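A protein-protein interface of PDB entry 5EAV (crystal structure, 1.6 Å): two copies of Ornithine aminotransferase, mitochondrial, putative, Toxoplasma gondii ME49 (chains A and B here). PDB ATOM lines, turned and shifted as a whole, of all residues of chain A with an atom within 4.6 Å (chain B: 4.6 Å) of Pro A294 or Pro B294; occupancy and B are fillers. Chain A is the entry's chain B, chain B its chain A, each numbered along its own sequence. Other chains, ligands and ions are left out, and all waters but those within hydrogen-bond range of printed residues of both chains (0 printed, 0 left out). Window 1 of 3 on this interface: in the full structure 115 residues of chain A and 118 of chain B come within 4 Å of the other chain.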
ATOM      1  N   MET A 133      -4.000  12.961  -0.694  1.00  0.00           N
ATOM      2  CA  MET A 133      -3.953  14.303  -0.146  1.00  0.00           C
ATOM      3  C   MET A 133      -4.264  15.260  -1.337  1.00  0.00           C
ATOM      4  O   MET A 133      -4.746  14.831  -2.381  1.00  0.00           O
ATOM      5  CB  MET A 133      -2.620  14.608   0.540  1.00  0.00           C
ATOM      6  CG  MET A 133      -2.254  13.685   1.746  1.00  0.00           C
ATOM      7  SD  MET A 133      -3.351  13.919   3.151  1.00  0.00           S
ATOM      8  CE  MET A 133      -2.794  15.382   3.948  1.00  0.00           C
ATOM      9  N   ASN A 134      -4.051  16.546  -1.122  1.00  0.00           N
ATOM     10  CA  ASN A 134      -4.388  17.526  -2.164  1.00  0.00           C
ATOM     11  C   ASN A 134      -3.217  18.076  -2.900  1.00  0.00           C
ATOM     12  O   ASN A 134      -3.189  18.018  -4.120  1.00  0.00           O
ATOM     13  CB  ASN A 134      -5.173  18.649  -1.509  1.00  0.00           C
ATOM     14  CG  ASN A 134      -6.309  18.128  -0.694  1.00  0.00           C
ATOM     15  OD1 ASN A 134      -7.354  17.780  -1.211  1.00  0.00           O
ATOM     16  ND2 ASN A 134      -6.101  18.063   0.602  1.00  0.00           N
ATOM     17  N   VAL A 293      -7.902  19.585 -10.768  1.00  0.00           N
ATOM     18  CA  VAL A 293      -8.113  19.839  -9.346  1.00  0.00           C
ATOM     19  C   VAL A 293      -6.862  19.306  -8.591  1.00  0.00           C
ATOM     20  O   VAL A 293      -6.183  18.352  -9.048  1.00  0.00           O
ATOM     21  CB  VAL A 293      -9.377  19.170  -8.785  1.00  0.00           C
ATOM     22  CG1 VAL A 293     -10.651  19.660  -9.464  1.00  0.00           C
ATOM     23  CG2 VAL A 293      -9.313  17.655  -8.954  1.00  0.00           C
ATOM     24  N   PRO A 294      -6.529  19.909  -7.447  1.00  0.00           N
ATOM     25  CA  PRO A 294      -5.385  19.450  -6.675  1.00  0.00           C
ATOM     26  C   PRO A 294      -5.581  18.050  -6.005  1.00  0.00           C
ATOM     27  O   PRO A 294      -6.522  17.867  -5.255  1.00  0.00           O
ATOM     28  CB  PRO A 294      -5.221  20.503  -5.561  1.00  0.00           C
ATOM     29  CG  PRO A 294      -6.201  21.551  -5.843  1.00  0.00           C
ATOM     30  CD  PRO A 294      -7.143  21.149  -6.902  1.00  0.00           C
ATOM     31  N   ILE A 295      -4.791  17.092  -6.419  1.00  0.00           N
ATOM     32  CA  ILE A 295      -4.777  15.765  -5.798  1.00  0.00           C
ATOM     33  C   ILE A 295      -3.367  15.236  -5.847  1.00  0.00           C
ATOM     34  O   ILE A 295      -2.706  15.318  -6.849  1.00  0.00           O
ATOM     35  CB  ILE A 295      -5.830  14.770  -6.339  1.00  0.00           C
ATOM     36  CG1 ILE A 295      -5.608  13.318  -5.829  1.00  0.00           C
ATOM     37  CG2 ILE A 295      -5.909  14.885  -7.803  1.00  0.00           C
ATOM     38  CD1 ILE A 295      -6.833  12.406  -5.938  1.00  0.00           C
ATOM     39  N   SER A 296      -2.945  14.659  -4.728  1.00  0.00           N
ATOM     40  CA  SER A 296      -1.636  14.092  -4.607  1.00  0.00           C
ATOM     41  C   SER A 296      -1.833  12.758  -3.862  1.00  0.00           C
ATOM     42  O   SER A 296      -2.924  12.467  -3.369  1.00  0.00           O
ATOM     43  CB  SER A 296      -0.719  15.019  -3.817  1.00  0.00           C
ATOM     44  OG  SER A 296      -1.218  15.185  -2.513  1.00  0.00           O
ATOM     45  N   PHE A 317     -10.262  17.648   2.278  1.00  0.00           N
ATOM     46  CA  PHE A 317     -10.509  17.303   0.926  1.00  0.00           C
ATOM     47  C   PHE A 317      -9.737  16.129   0.397  1.00  0.00           C
ATOM     48  O   PHE A 317      -9.994  15.716  -0.718  1.00  0.00           O
ATOM     49  CB  PHE A 317     -10.277  18.537  -0.011  1.00  0.00           C
ATOM     50  CG  PHE A 317     -11.337  19.569   0.094  1.00  0.00           C
ATOM     51  CD1 PHE A 317     -11.289  20.568   1.078  1.00  0.00           C
ATOM     52  CD2 PHE A 317     -12.395  19.572  -0.808  1.00  0.00           C
ATOM     53  CE1 PHE A 317     -12.282  21.531   1.166  1.00  0.00           C
ATOM     54  CE2 PHE A 317     -13.411  20.517  -0.681  1.00  0.00           C
ATOM     55  CZ  PHE A 317     -13.343  21.489   0.291  1.00  0.00           C
ATOM     56  N   MET B 133      -4.653  29.775  -1.733  1.00  0.00           N
ATOM     57  CA  MET B 133      -3.974  28.500  -1.569  1.00  0.00           C
ATOM     58  C   MET B 133      -5.041  27.400  -1.771  1.00  0.00           C
ATOM     59  O   MET B 133      -6.135  27.672  -2.257  1.00  0.00           O
ATOM     60  CB  MET B 133      -3.291  28.423  -0.154  1.00  0.00           C
ATOM     61  CG  MET B 133      -2.165  29.458   0.087  1.00  0.00           C
ATOM     62  SD  MET B 133      -0.758  29.287  -1.020  1.00  0.00           S
ATOM     63  CE  MET B 133      -0.067  27.810  -0.306  1.00  0.00           C
ATOM     64  N   ASN B 134      -4.736  26.160  -1.360  1.00  0.00           N
ATOM     65  CA  ASN B 134      -5.669  25.064  -1.630  1.00  0.00           C
ATOM     66  C   ASN B 134      -6.336  24.535  -0.384  1.00  0.00           C
ATOM     67  O   ASN B 134      -7.535  24.375  -0.350  1.00  0.00           O
ATOM     68  CB  ASN B 134      -4.919  23.938  -2.384  1.00  0.00           C
ATOM     69  CG  ASN B 134      -4.166  24.434  -3.590  1.00  0.00           C
ATOM     70  OD1 ASN B 134      -4.773  24.672  -4.591  1.00  0.00           O
ATOM     71  ND2 ASN B 134      -2.871  24.649  -3.465  1.00  0.00           N
ATOM     72  N   VAL B 293     -13.989  21.811  -4.661  1.00  0.00           N
ATOM     73  CA  VAL B 293     -12.542  21.691  -4.944  1.00  0.00           C
ATOM     74  C   VAL B 293     -11.869  22.422  -3.793  1.00  0.00           C
ATOM     75  O   VAL B 293     -12.443  23.387  -3.231  1.00  0.00           O
ATOM     76  CB  VAL B 293     -12.097  22.364  -6.269  1.00  0.00           C
ATOM     77  CG1 VAL B 293     -12.638  21.671  -7.527  1.00  0.00           C
ATOM     78  CG2 VAL B 293     -12.504  23.809  -6.297  1.00  0.00           C
ATOM     79  N   PRO B 294     -10.678  22.001  -3.412  1.00  0.00           N
ATOM     80  CA  PRO B 294     -10.032  22.676  -2.308  1.00  0.00           C
ATOM     81  C   PRO B 294      -9.486  24.059  -2.678  1.00  0.00           C
ATOM     82  O   PRO B 294      -8.672  24.156  -3.555  1.00  0.00           O
ATOM     83  CB  PRO B 294      -8.868  21.763  -1.929  1.00  0.00           C
ATOM     84  CG  PRO B 294      -8.784  20.736  -2.949  1.00  0.00           C
ATOM     85  CD  PRO B 294      -9.972  20.766  -3.839  1.00  0.00           C
ATOM     86  N   ILE B 295     -10.025  25.078  -2.038  1.00  0.00           N
ATOM     87  CA  ILE B 295      -9.506  26.443  -2.179  1.00  0.00           C
ATOM     88  C   ILE B 295      -9.576  27.125  -0.828  1.00  0.00           C
ATOM     89  O   ILE B 295     -10.532  26.948  -0.088  1.00  0.00           O
ATOM     90  CB  ILE B 295     -10.108  27.234  -3.376  1.00  0.00           C
ATOM     91  CG1 ILE B 295      -9.748  28.701  -3.293  1.00  0.00           C
ATOM     92  CG2 ILE B 295     -11.598  27.007  -3.528  1.00  0.00           C
ATOM     93  CD1 ILE B 295      -9.970  29.542  -4.573  1.00  0.00           C
ATOM     94  N   SER B 296      -8.492  27.794  -0.477  1.00  0.00           N
ATOM     95  CA  SER B 296      -8.394  28.536   0.756  1.00  0.00           C
ATOM     96  C   SER B 296      -7.812  29.895   0.505  1.00  0.00           C
ATOM     97  O   SER B 296      -7.301  30.146  -0.580  1.00  0.00           O
ATOM     98  CB  SER B 296      -7.589  27.745   1.796  1.00  0.00           C
ATOM     99  OG  SER B 296      -6.189  27.657   1.432  1.00  0.00           O
ATOM    100  N   PHE B 317      -1.250  24.817  -7.544  1.00  0.00           N
ATOM    101  CA  PHE B 317      -2.685  25.008  -7.811  1.00  0.00           C
ATOM    102  C   PHE B 317      -3.326  26.235  -7.169  1.00  0.00           C
ATOM    103  O   PHE B 317      -4.459  26.512  -7.404  1.00  0.00           O
ATOM    104  CB  PHE B 317      -3.440  23.730  -7.435  1.00  0.00           C
ATOM    105  CG  PHE B 317      -3.243  22.595  -8.389  1.00  0.00           C
ATOM    106  CD1 PHE B 317      -2.197  21.696  -8.229  1.00  0.00           C
ATOM    107  CD2 PHE B 317      -4.157  22.366  -9.388  1.00  0.00           C
ATOM    108  CE1 PHE B 317      -2.023  20.635  -9.123  1.00  0.00           C
ATOM    109  CE2 PHE B 317      -4.005  21.299 -10.261  1.00  0.00           C
ATOM    110  CZ  PHE B 317      -2.939  20.446 -10.114  1.00  0.00           C
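O of Phe A317 lies close to OD1 of Asn A134, at 3.4 Å. N of Ile A295 sits at hydrogen-bond distance from O of Asn A134 (3.0 Å). The side-chain amide oxygen (OD1) of Asn B134 lies close to the backbone carbonyl oxygen (O) of Phe B317, 3.4 Å away. The backbone carbonyl oxygen of Asn A134 lies within hydrogen-bond range of the backbone NH of Ser A296, 3.4 Å away. The backbone NH (N) of Asn B134 lies within hydrogen-bond range of the side-chain hydroxyl (OG) of Ser B296 (3.5 Å). O of Asn B134 lies within hydrogen-bond range of N of Ile B295.
Asn A134 touches Pro B294. Val A293 touches Val B293 (CG1 to CG1, 3.4 Å). Val A293 touches Phe B317 (O to CE2, 3.9 Å). OD1 of Asn B134 touches CG of Pro A294, at 3.7 Å. CG of Pro A294 touches CG of Pro B294, 3.96 Å away. Phe B317 touches Pro A294. O of Val B293 touches CE2 of Phe A317 (3.96 Å). Phe A317 touches Pro B294 (CG to CB, 3.9 Å).
Asn A134 touches Pro B294, and with the chains exchanged Pro A294 touches Asn B134. Val A293 touches its own counterpart, Val B293. Pro A294 touches its own counterpart, Pro B294. Pro A294 touches Phe B317, and with the chains exchanged Phe A317 touches Pro B294. Of the 8 pairs that touch across the chains among the printed residues, 8 have their exchanged pair printed and touching as well.
Printed residues of chain B within 4 Å of Asn A134: Pro B294. Pro A294 touches just these residues of chain B: Asn B134, Pro B294 and Phe B317. Printed residues of chain B within 4 Å of Phe A317: Val B293 and Pro B294. Printed residues of chain A within 4 Å of Asn B134: Pro A294. Of the printed residues of chain A, Val B293 touches Val A293 (3.4 Å) and Phe A317 (3.96 Å). Pro B294 touches three residues of chain A. Of the printed residues of chain A, Phe B317 touches Val A293 and Pro A294. The nearest printed residue of chain B that does not touch Pro A294 is Val B293 (5.1 Å). The nearest printed residue of chain A that does not touch Pro B294 is Val A293 (5.2 Å).
Hydrophobic or aromatic side chains of chain B that line the printed part of chain A: Val B293, Pro B294 and Phe B317. Of the 7 printed residues of chain A, 4 touch a printed residue of chain B. Printed residues of chain A that touch a printed residue of chain B: Asn A134, Val A293, Pro A294 and Phe A317.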
